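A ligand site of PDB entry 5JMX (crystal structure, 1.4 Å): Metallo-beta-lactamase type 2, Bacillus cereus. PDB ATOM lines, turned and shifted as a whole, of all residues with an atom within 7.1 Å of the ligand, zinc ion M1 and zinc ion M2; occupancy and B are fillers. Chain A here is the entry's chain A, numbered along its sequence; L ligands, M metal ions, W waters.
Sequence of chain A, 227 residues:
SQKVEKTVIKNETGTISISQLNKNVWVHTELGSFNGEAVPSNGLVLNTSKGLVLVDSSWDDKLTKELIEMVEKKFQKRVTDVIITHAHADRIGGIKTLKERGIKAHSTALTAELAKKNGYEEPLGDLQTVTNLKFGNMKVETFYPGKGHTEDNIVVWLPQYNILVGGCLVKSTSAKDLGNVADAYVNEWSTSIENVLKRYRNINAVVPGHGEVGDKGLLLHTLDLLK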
ATOM      1  N   PRO A  40       7.513  -8.307  -1.377  1.00  0.00           N
ATOM      2  CA  PRO A  40       7.107  -7.586  -0.172  1.00  0.00           C
ATOM      3  C   PRO A  40       7.038  -6.096  -0.429  1.00  0.00           C
ATOM      4  O   PRO A  40       7.754  -5.557  -1.281  1.00  0.00           O
ATOM      5  CB  PRO A  40       8.241  -7.892   0.807  1.00  0.00           C
ATOM      6  CG  PRO A  40       9.410  -8.006  -0.042  1.00  0.00           C
ATOM      7  CD  PRO A  40       8.943  -8.619  -1.347  1.00  0.00           C
ATOM      8  N   SER A  41       6.168  -5.462   0.334  1.00  0.00           N
ATOM      9  CA  SER A  41       5.973  -4.019   0.277  1.00  0.00           C
ATOM     10  C   SER A  41       5.838  -3.501   1.701  1.00  0.00           C
ATOM     11  O   SER A  41       5.224  -4.186   2.542  1.00  0.00           O
ATOM     12  CB  SER A  41       4.681  -3.721  -0.495  1.00  0.00           C
ATOM     13  OG  SER A  41       4.253  -2.381  -0.304  1.00  0.00           O
ATOM     14  N   TRP A  59      -1.360  -4.257  -1.392  1.00  0.00           N
ATOM     15  CA  TRP A  59      -1.496  -4.602  -2.801  1.00  0.00           C
ATOM     16  C   TRP A  59      -2.948  -4.728  -3.245  1.00  0.00           C
ATOM     17  O   TRP A  59      -3.254  -4.499  -4.412  1.00  0.00           O
ATOM     18  CB  TRP A  59      -0.834  -5.946  -3.010  1.00  0.00           C
ATOM     19  CG  TRP A  59       0.637  -5.975  -2.744  1.00  0.00           C
ATOM     20  CD1 TRP A  59       1.271  -6.336  -1.592  1.00  0.00           C
ATOM     21  CD2 TRP A  59       1.672  -5.654  -3.684  1.00  0.00           C
ATOM     22  NE1 TRP A  59       2.644  -6.281  -1.763  1.00  0.00           N
ATOM     23  CE2 TRP A  59       2.910  -5.855  -3.034  1.00  0.00           C
ATOM     24  CE3 TRP A  59       1.665  -5.209  -4.994  1.00  0.00           C
ATOM     25  CZ2 TRP A  59       4.132  -5.630  -3.669  1.00  0.00           C
ATOM     26  CZ3 TRP A  59       2.882  -4.987  -5.622  1.00  0.00           C
ATOM     27  CH2 TRP A  59       4.088  -5.188  -4.954  1.00  0.00           C
ATOM     28  N   HIS A  86       1.778   7.068  -3.453  1.00  0.00           N
ATOM     29  CA  HIS A  86       1.627   7.206  -4.899  1.00  0.00           C
ATOM     30  C   HIS A  86       0.533   6.263  -5.357  1.00  0.00           C
ATOM     31  O   HIS A  86      -0.019   5.492  -4.582  1.00  0.00           O
ATOM     32  CB  HIS A  86       2.938   7.064  -5.694  1.00  0.00           C
ATOM     33  CG  HIS A  86       3.526   5.684  -5.752  1.00  0.00           C
ATOM     34  ND1 HIS A  86       4.352   5.219  -4.738  1.00  0.00           N
ATOM     35  CD2 HIS A  86       3.610   4.766  -6.746  1.00  0.00           C
ATOM     36  CE1 HIS A  86       4.802   4.021  -5.063  1.00  0.00           C
ATOM     37  NE2 HIS A  86       4.361   3.707  -6.270  1.00  0.00           N
ATOM     38  N   ALA A  87       0.166   6.366  -6.630  1.00  0.00           N
ATOM     39  CA  ALA A  87      -1.002   5.656  -7.126  1.00  0.00           C
ATOM     40  C   ALA A  87      -0.688   4.331  -7.814  1.00  0.00           C
ATOM     41  O   ALA A  87      -1.341   3.965  -8.791  1.00  0.00           O
ATOM     42  CB  ALA A  87      -1.766   6.574  -8.090  1.00  0.00           C
ATOM     43  N   HIS A  88       0.260   3.541  -7.330  1.00  0.00           N
ATOM     44  CA  HIS A  88       0.432   2.174  -7.777  1.00  0.00           C
ATOM     45  C   HIS A  88      -0.218   1.219  -6.771  1.00  0.00           C
ATOM     46  O   HIS A  88      -0.458   1.574  -5.629  1.00  0.00           O
ATOM     47  CB  HIS A  88       1.930   1.868  -7.862  1.00  0.00           C
ATOM     48  CG  HIS A  88       2.616   2.379  -9.074  1.00  0.00           C
ATOM     49  ND1 HIS A  88       3.986   2.546  -9.147  1.00  0.00           N
ATOM     50  CD2 HIS A  88       2.140   2.695 -10.304  1.00  0.00           C
ATOM     51  CE1 HIS A  88       4.309   2.974 -10.357  1.00  0.00           C
ATOM     52  NE2 HIS A  88       3.212   3.042 -11.088  1.00  0.00           N
ATOM     53  N   ALA A  89      -0.446  -0.037  -7.194  1.00  0.00           N
ATOM     54  CA  ALA A  89      -1.281  -0.953  -6.425  1.00  0.00           C
ATOM     55  C   ALA A  89      -0.676  -1.283  -5.071  1.00  0.00           C
ATOM     56  O   ALA A  89      -1.406  -1.503  -4.116  1.00  0.00           O
ATOM     57  CB  ALA A  89      -1.490  -2.245  -7.217  1.00  0.00           C
ATOM     58  N   ASP A  90       0.654  -1.350  -4.956  1.00  0.00           N
ATOM     59  CA  ASP A  90       1.226  -1.638  -3.645  1.00  0.00           C
ATOM     60  C   ASP A  90       0.883  -0.572  -2.611  1.00  0.00           C
ATOM     61  O   ASP A  90       0.870  -0.857  -1.405  1.00  0.00           O
ATOM     62  CB  ASP A  90       2.744  -1.894  -3.749  1.00  0.00           C
ATOM     63  CG  ASP A  90       3.532  -0.685  -4.212  1.00  0.00           C
ATOM     64  OD1 ASP A  90       3.011   0.139  -4.995  1.00  0.00           O
ATOM     65  OD2 ASP A  90       4.755  -0.602  -3.864  1.00  0.00           O
ATOM     66  N   ARG A  91       0.594   0.646  -3.040  1.00  0.00           N
ATOM     67  CA  ARG A  91       0.263   1.741  -2.136  1.00  0.00           C
ATOM     68  C   ARG A  91      -1.236   1.892  -1.971  1.00  0.00           C
ATOM     69  O   ARG A  91      -1.703   2.170  -0.861  1.00  0.00           O
ATOM     70  CB  ARG A  91       0.816   3.075  -2.687  1.00  0.00           C
ATOM     71  CG  ARG A  91       2.278   3.083  -3.103  1.00  0.00           C
ATOM     72  CD  ARG A  91       3.177   2.943  -1.905  1.00  0.00           C
ATOM     73  NE  ARG A  91       3.855   1.667  -1.894  1.00  0.00           N
ATOM     74  CZ  ARG A  91       4.572   1.203  -0.875  1.00  0.00           C
ATOM     75  NH1 ARG A  91       4.665   1.887   0.247  1.00  0.00           N
ATOM     76  NH2 ARG A  91       5.210   0.064  -1.001  1.00  0.00           N
ATOM     77  N   HIS A 149      10.321   7.828  -8.860  1.00  0.00           N
ATOM     78  CA  HIS A 149       9.767   6.526  -9.169  1.00  0.00           C
ATOM     79  C   HIS A 149       8.454   6.671  -9.923  1.00  0.00           C
ATOM     80  O   HIS A 149       8.158   5.887 -10.836  1.00  0.00           O
ATOM     81  CB  HIS A 149       9.530   5.804  -7.850  1.00  0.00           C
ATOM     82  CG  HIS A 149       8.623   4.620  -7.969  1.00  0.00           C
ATOM     83  ND1 HIS A 149       8.967   3.483  -8.658  1.00  0.00           N
ATOM     84  CD2 HIS A 149       7.351   4.421  -7.540  1.00  0.00           C
ATOM     85  CE1 HIS A 149       7.983   2.616  -8.616  1.00  0.00           C
ATOM     86  NE2 HIS A 149       6.981   3.166  -7.940  1.00  0.00           N
ATOM     87  N   THR A 150       7.649   7.662  -9.534  1.00  0.00           N
ATOM     88  CA  THR A 150       6.497   8.082 -10.300  1.00  0.00           C
ATOM     89  C   THR A 150       6.430   9.593 -10.303  1.00  0.00           C
ATOM     90  O   THR A 150       7.205  10.292  -9.637  1.00  0.00           O
ATOM     91  CB  THR A 150       5.192   7.568  -9.707  1.00  0.00           C
ATOM     92  OG1 THR A 150       5.104   8.082  -8.365  1.00  0.00           O
ATOM     93  CG2 THR A 150       5.109   6.075  -9.778  1.00  0.00           C
ATOM     94  N   GLY A 167       9.155   5.456   0.789  1.00  0.00           N
ATOM     95  CA  GLY A 167       8.318   4.875  -0.194  1.00  0.00           C
ATOM     96  C   GLY A 167       9.158   4.396  -1.363  1.00  0.00           C
ATOM     97  O   GLY A 167      10.350   4.097  -1.243  1.00  0.00           O
ATOM     98  N   CYS A 168       8.501   4.305  -2.517  1.00  0.00           N
ATOM     99  CA  CYS A 168       9.149   3.667  -3.640  1.00  0.00           C
ATOM    100  C   CYS A 168      10.127   4.578  -4.334  1.00  0.00           C
ATOM    101  O   CYS A 168      10.880   4.105  -5.199  1.00  0.00           O
ATOM    102  CB  CYS A 168       8.109   3.039  -4.543  1.00  0.00           C
ATOM    103  SG  CYS A 168       7.041   1.889  -3.559  1.00  0.00           S
ATOM    104  N   LEU A 169      10.187   5.863  -3.931  1.00  0.00           N
ATOM    105  CA  LEU A 169      11.276   6.743  -4.322  1.00  0.00           C
ATOM    106  C   LEU A 169      12.625   6.250  -3.828  1.00  0.00           C
ATOM    107  O   LEU A 169      13.660   6.594  -4.428  1.00  0.00           O
ATOM    108  CB  LEU A 169      11.012   8.138  -3.750  1.00  0.00           C
ATOM    109  CG  LEU A 169      11.952   9.243  -4.129  1.00  0.00           C
ATOM    110  CD1 LEU A 169      11.655   9.679  -5.550  1.00  0.00           C
ATOM    111  CD2 LEU A 169      11.796  10.403  -3.144  1.00  0.00           C
ATOM    112  N   VAL A 170      12.677   5.475  -2.753  1.00  0.00           N
ATOM    113  CA  VAL A 170      13.907   5.067  -2.095  1.00  0.00           C
ATOM    114  C   VAL A 170      14.031   3.559  -2.240  1.00  0.00           C
ATOM    115  O   VAL A 170      13.135   2.813  -1.843  1.00  0.00           O
ATOM    116  CB  VAL A 170      13.901   5.504  -0.618  1.00  0.00           C
ATOM    117  CG1 VAL A 170      15.173   5.035   0.070  1.00  0.00           C
ATOM    118  CG2 VAL A 170      13.780   7.006  -0.511  1.00  0.00           C
ATOM    119  N   LYS A 171      15.165   3.107  -2.787  1.00  0.00           N
ATOM    120  CA  LYS A 171      15.451   1.703  -2.942  1.00  0.00           C
ATOM    121  C   LYS A 171      16.212   1.173  -1.746  1.00  0.00           C
ATOM    122  O   LYS A 171      17.032   1.858  -1.143  1.00  0.00           O
ATOM    123  CB  LYS A 171      16.298   1.475  -4.204  1.00  0.00           C
ATOM    124  CG  LYS A 171      15.742   2.100  -5.461  1.00  0.00           C
ATOM    125  CD  LYS A 171      14.340   1.671  -5.831  1.00  0.00           C
ATOM    126  CE  LYS A 171      14.199   0.208  -6.113  1.00  0.00           C
ATOM    127  NZ  LYS A 171      12.820  -0.080  -6.728  1.00  0.00           N
ATOM    128  N   LEU A 178      16.713  -0.136 -10.507  1.00  0.00           N
ATOM    129  CA  LEU A 178      15.613   0.735 -10.123  1.00  0.00           C
ATOM    130  C   LEU A 178      14.256   0.054 -10.174  1.00  0.00           C
ATOM    131  O   LEU A 178      13.269   0.681  -9.793  1.00  0.00           O
ATOM    132  CB  LEU A 178      15.603   1.978 -11.008  1.00  0.00           C
ATOM    133  CG  LEU A 178      16.829   2.874 -10.865  1.00  0.00           C
ATOM    134  CD1 LEU A 178      16.891   3.851 -12.032  1.00  0.00           C
ATOM    135  CD2 LEU A 178      16.829   3.590  -9.533  1.00  0.00           C
ATOM    136  N   GLY A 179      14.176  -1.190 -10.648  1.00  0.00           N
ATOM    137  CA  GLY A 179      12.884  -1.845 -10.760  1.00  0.00           C
ATOM    138  C   GLY A 179      12.137  -1.370 -11.991  1.00  0.00           C
ATOM    139  O   GLY A 179      12.731  -0.947 -12.985  1.00  0.00           O
ATOM    140  N   ASN A 180      10.813  -1.435 -11.940  1.00  0.00           N
ATOM    141  CA  ASN A 180      10.003  -1.041 -13.092  1.00  0.00           C
ATOM    142  C   ASN A 180       9.994   0.470 -13.194  1.00  0.00           C
ATOM    143  O   ASN A 180       9.559   1.158 -12.252  1.00  0.00           O
ATOM    144  CB  ASN A 180       8.588  -1.604 -12.940  1.00  0.00           C
ATOM    145  CG  ASN A 180       7.723  -1.375 -14.172  1.00  0.00           C
ATOM    146  OD1 ASN A 180       7.755  -0.314 -14.787  1.00  0.00           O
ATOM    147  ND2 ASN A 180       6.957  -2.398 -14.564  1.00  0.00           N
ATOM    148  N   VAL A 181      10.487   1.008 -14.295  1.00  0.00           N
ATOM    149  CA  VAL A 181      10.631   2.442 -14.501  1.00  0.00           C
ATOM    150  C   VAL A 181       9.619   2.959 -15.526  1.00  0.00           C
ATOM    151  O   VAL A 181       9.758   4.075 -16.031  1.00  0.00           O
ATOM    152  CB  VAL A 181      12.079   2.833 -14.852  1.00  0.00           C
ATOM    153  CG1 VAL A 181      12.998   2.585 -13.655  1.00  0.00           C
ATOM    154  CG2 VAL A 181      12.567   2.077 -16.116  1.00  0.00           C
ATOM    155  N   ALA A 182       8.585   2.171 -15.820  1.00  0.00           N
ATOM    156  CA  ALA A 182       7.611   2.556 -16.830  1.00  0.00           C
ATOM    157  C   ALA A 182       6.970   3.897 -16.488  1.00  0.00           C
ATOM    158  O   ALA A 182       6.680   4.711 -17.365  1.00  0.00           O
ATOM    159  CB  ALA A 182       6.533   1.487 -16.954  1.00  0.00           C
ATOM    160  N   ASP A 183       6.720   4.138 -15.207  1.00  0.00           N
ATOM    161  CA  ASP A 183       6.110   5.388 -14.791  1.00  0.00           C
ATOM    162  C   ASP A 183       7.104   6.362 -14.188  1.00  0.00           C
ATOM    163  O   ASP A 183       6.676   7.343 -13.557  1.00  0.00           O
ATOM    164  CB  ASP A 183       4.985   5.107 -13.796  1.00  0.00           C
ATOM    165  CG  ASP A 183       3.870   4.302 -14.403  1.00  0.00           C
ATOM    166  OD1 ASP A 183       3.607   4.414 -15.632  1.00  0.00           O
ATOM    167  OD2 ASP A 183       3.183   3.570 -13.661  1.00  0.00           O
ATOM    168  N   ALA A 184       8.410   6.148 -14.360  1.00  0.00           N
ATOM    169  CA  ALA A 184       9.427   6.876 -13.644  1.00  0.00           C
ATOM    170  C   ALA A 184      10.001   7.999 -14.491  1.00  0.00           C
ATOM    171  O   ALA A 184       9.786   8.079 -15.702  1.00  0.00           O
ATOM    172  CB  ALA A 184      10.542   5.927 -13.223  1.00  0.00           C
ATOM    173  N   TRP A 189      14.642  12.052 -10.871  1.00  0.00           N
ATOM    174  CA  TRP A 189      14.640  11.282  -9.619  1.00  0.00           C
ATOM    175  C   TRP A 189      15.817  11.654  -8.732  1.00  0.00           C
ATOM    176  O   TRP A 189      15.669  11.751  -7.512  1.00  0.00           O
ATOM    177  CB  TRP A 189      14.649   9.801 -10.010  1.00  0.00           C
ATOM    178  CG  TRP A 189      14.328   8.792  -8.967  1.00  0.00           C
ATOM    179  CD1 TRP A 189      14.392   8.913  -7.582  1.00  0.00           C
ATOM    180  CD2 TRP A 189      13.905   7.457  -9.231  1.00  0.00           C
ATOM    181  NE1 TRP A 189      14.058   7.708  -7.008  1.00  0.00           N
ATOM    182  CE2 TRP A 189      13.718   6.818  -7.987  1.00  0.00           C
ATOM    183  CE3 TRP A 189      13.625   6.763 -10.399  1.00  0.00           C
ATOM    184  CZ2 TRP A 189      13.303   5.479  -7.904  1.00  0.00           C
ATOM    185  CZ3 TRP A 189      13.230   5.450 -10.331  1.00  0.00           C
ATOM    186  CH2 TRP A 189      13.039   4.816  -9.075  1.00  0.00           C
ATOM    187  N   GLY A 209      10.179   1.602   0.122  1.00  0.00           N
ATOM    188  CA  GLY A 209       8.943   1.004  -0.291  1.00  0.00           C
ATOM    189  C   GLY A 209       8.968  -0.512  -0.255  1.00  0.00           C
ATOM    190  O   GLY A 209       7.934  -1.146  -0.015  1.00  0.00           O
ATOM    191  N   HIS A 210      10.129  -1.115  -0.519  1.00  0.00           N
ATOM    192  CA  HIS A 210      10.328  -2.553  -0.519  1.00  0.00           C
ATOM    193  C   HIS A 210      11.709  -2.808   0.078  1.00  0.00           C
ATOM    194  O   HIS A 210      12.660  -2.107  -0.277  1.00  0.00           O
ATOM    195  CB  HIS A 210      10.265  -3.112  -1.971  1.00  0.00           C
ATOM    196  CG  HIS A 210       9.074  -2.624  -2.737  1.00  0.00           C
ATOM    197  ND1 HIS A 210       7.868  -3.312  -2.757  1.00  0.00           N
ATOM    198  CD2 HIS A 210       8.858  -1.476  -3.426  1.00  0.00           C
ATOM    199  CE1 HIS A 210       6.988  -2.620  -3.467  1.00  0.00           C
ATOM    200  NE2 HIS A 210       7.551  -1.492  -3.864  1.00  0.00           N
HETATM  201  O1  LIG L   1       8.380   0.211  -6.007  1.00  0.00           O
HETATM  202  C1  LIG L   1       8.290  -0.296  -7.162  1.00  0.00           C
HETATM  203  O2  LIG L   1       9.312  -0.689  -7.795  1.00  0.00           O
HETATM  204  C2  LIG L   1       6.940  -0.273  -7.883  1.00  0.00           C
HETATM  205  C3  LIG L   1       6.884  -0.518  -9.232  1.00  0.00           C
HETATM  206  C4  LIG L   1       5.728  -0.432 -10.129  1.00  0.00           C
HETATM  207  C5  LIG L   1       4.439  -0.952  -9.897  1.00  0.00           C
HETATM  208  C6  LIG L   1       3.395  -0.818 -10.806  1.00  0.00           C
HETATM  209  C7  LIG L   1       3.675  -0.144 -12.005  1.00  0.00           C
HETATM  210  F1  LIG L   1       2.658   0.012 -12.926  1.00  0.00           F
HETATM  211  C8  LIG L   1       4.873   0.391 -12.313  1.00  0.00           C
HETATM  212  C9  LIG L   1       5.895   0.237 -11.376  1.00  0.00           C
HETATM  213  S1  LIG L   1       5.516   0.099  -6.966  1.00  0.00           S
HETATM  214 ZN    ZN M   1       6.538   0.068  -4.818  1.00  0.00          ZN
HETATM  215 ZN    ZN M   2       5.205   2.312  -7.513  1.00  0.00          ZN
HETATM  216  O   HOH W   1       9.616  -2.565  -9.727  1.00  0.00           O
HETATM  217  O   HOH W   2      10.842   1.203  -5.320  1.00  0.00           O
HETATM  218  O   HOH W   3       2.575  -1.640  -7.120  1.00  0.00           O
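The side-chain amino group of Lys 171 lies within salt-bridge range of an oxygen (O2) of the ligand, at 3.7 Å.
A ring nitrogen (NE2) of His 88 is in hydrogen-bond range of the side-chain carboxylate (OD2) of Asp 183, 2.6 Å away. The backbone carbonyl oxygen (O) of Pro 40 sits at hydrogen-bond distance from a ring nitrogen (ND1) of His 210 (2.7 Å). The guanidinium group (NE) of Arg 91 is in salt-bridge range of the side-chain carboxylate (OD1) of Asp 90. The side-chain sulfur (SG) of Cys 168 sits close to the guanidinium group (NE) of Arg 91 (3.6 Å). The backbone NH (N) of Ala 182 lies within hydrogen-bond range of the side-chain amide oxygen (OD1) of Asn 180. The side-chain amino group of Lys 171 lies within hydrogen-bond range of the backbone carbonyl oxygen of Leu 178 (3.2 Å).
CB of Asn 180 touches C9 of the ligand (3.6 Å). Asp 183 touches the ligand (OD2 to F1, 3.7 Å). Hydrophobic or aromatic side chains within 4 Å of the ligand: His 88, His 149 and His 210. Nine residues have an atom within 4 Å of the ligand: His 86, His 88, Asp 90, His 149, Cys 168, Lys 171, Asn 180, Asp 183 and His 210. The nearest printed residue that does not touch the ligand is Leu 178 (4.6 Å).
Three residues have an atom within 4 Å of zinc ion M1: Asp 90, Cys 168 and His 210. The nearest printed residue that does not touch zinc ion M1 is Arg 91 (4.04 Å).
Four residues have an atom within 4 Å of zinc ion M2: His 86, His 88, Asp 90 and His 149. The nearest printed residue that does not touch zinc ion M2 is Cys 168 (4.2 Å).
NE2 of His 210 binds zinc ion M1, at 2.1 Å. OD2 of Asp 90 is bound to zinc ion M1. An oxygen (O1) of the ligand binds zinc ion M1 (2.2 Å). SG of Cys 168 binds zinc ion M1 (2.3 Å). S1 of the ligand binds zinc ion M1 (2.4 Å).
Zinc ion M2 is bound by NE2 of His 149 (2.0 Å). Zinc ion M2 is bound by a ring nitrogen (NE2) of His 86 (2.1 Å). ND1 of His 88 is bound to zinc ion M2 (2.1 Å). Zinc ion M2 is bound by S1 of the ligand (2.3 Å). Zinc ion M2 has four donor atoms within binding distance.
Water W1 lies within hydrogen-bond range of an oxygen (O2) of the ligand (2.7 Å) and the backbone NH of Asn 180 (2.8 Å). Water W2 lies within hydrogen-bond range of the side-chain amino group of Lys 171 (2.7 Å), the backbone carbonyl oxygen of Cys 168 (2.9 Å) and an oxygen (O2) of the ligand (3.5 Å). Water W3 bridges OD1 of Asp 90 (2.8 Å) and N of Ala 89 (3.4 Å).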
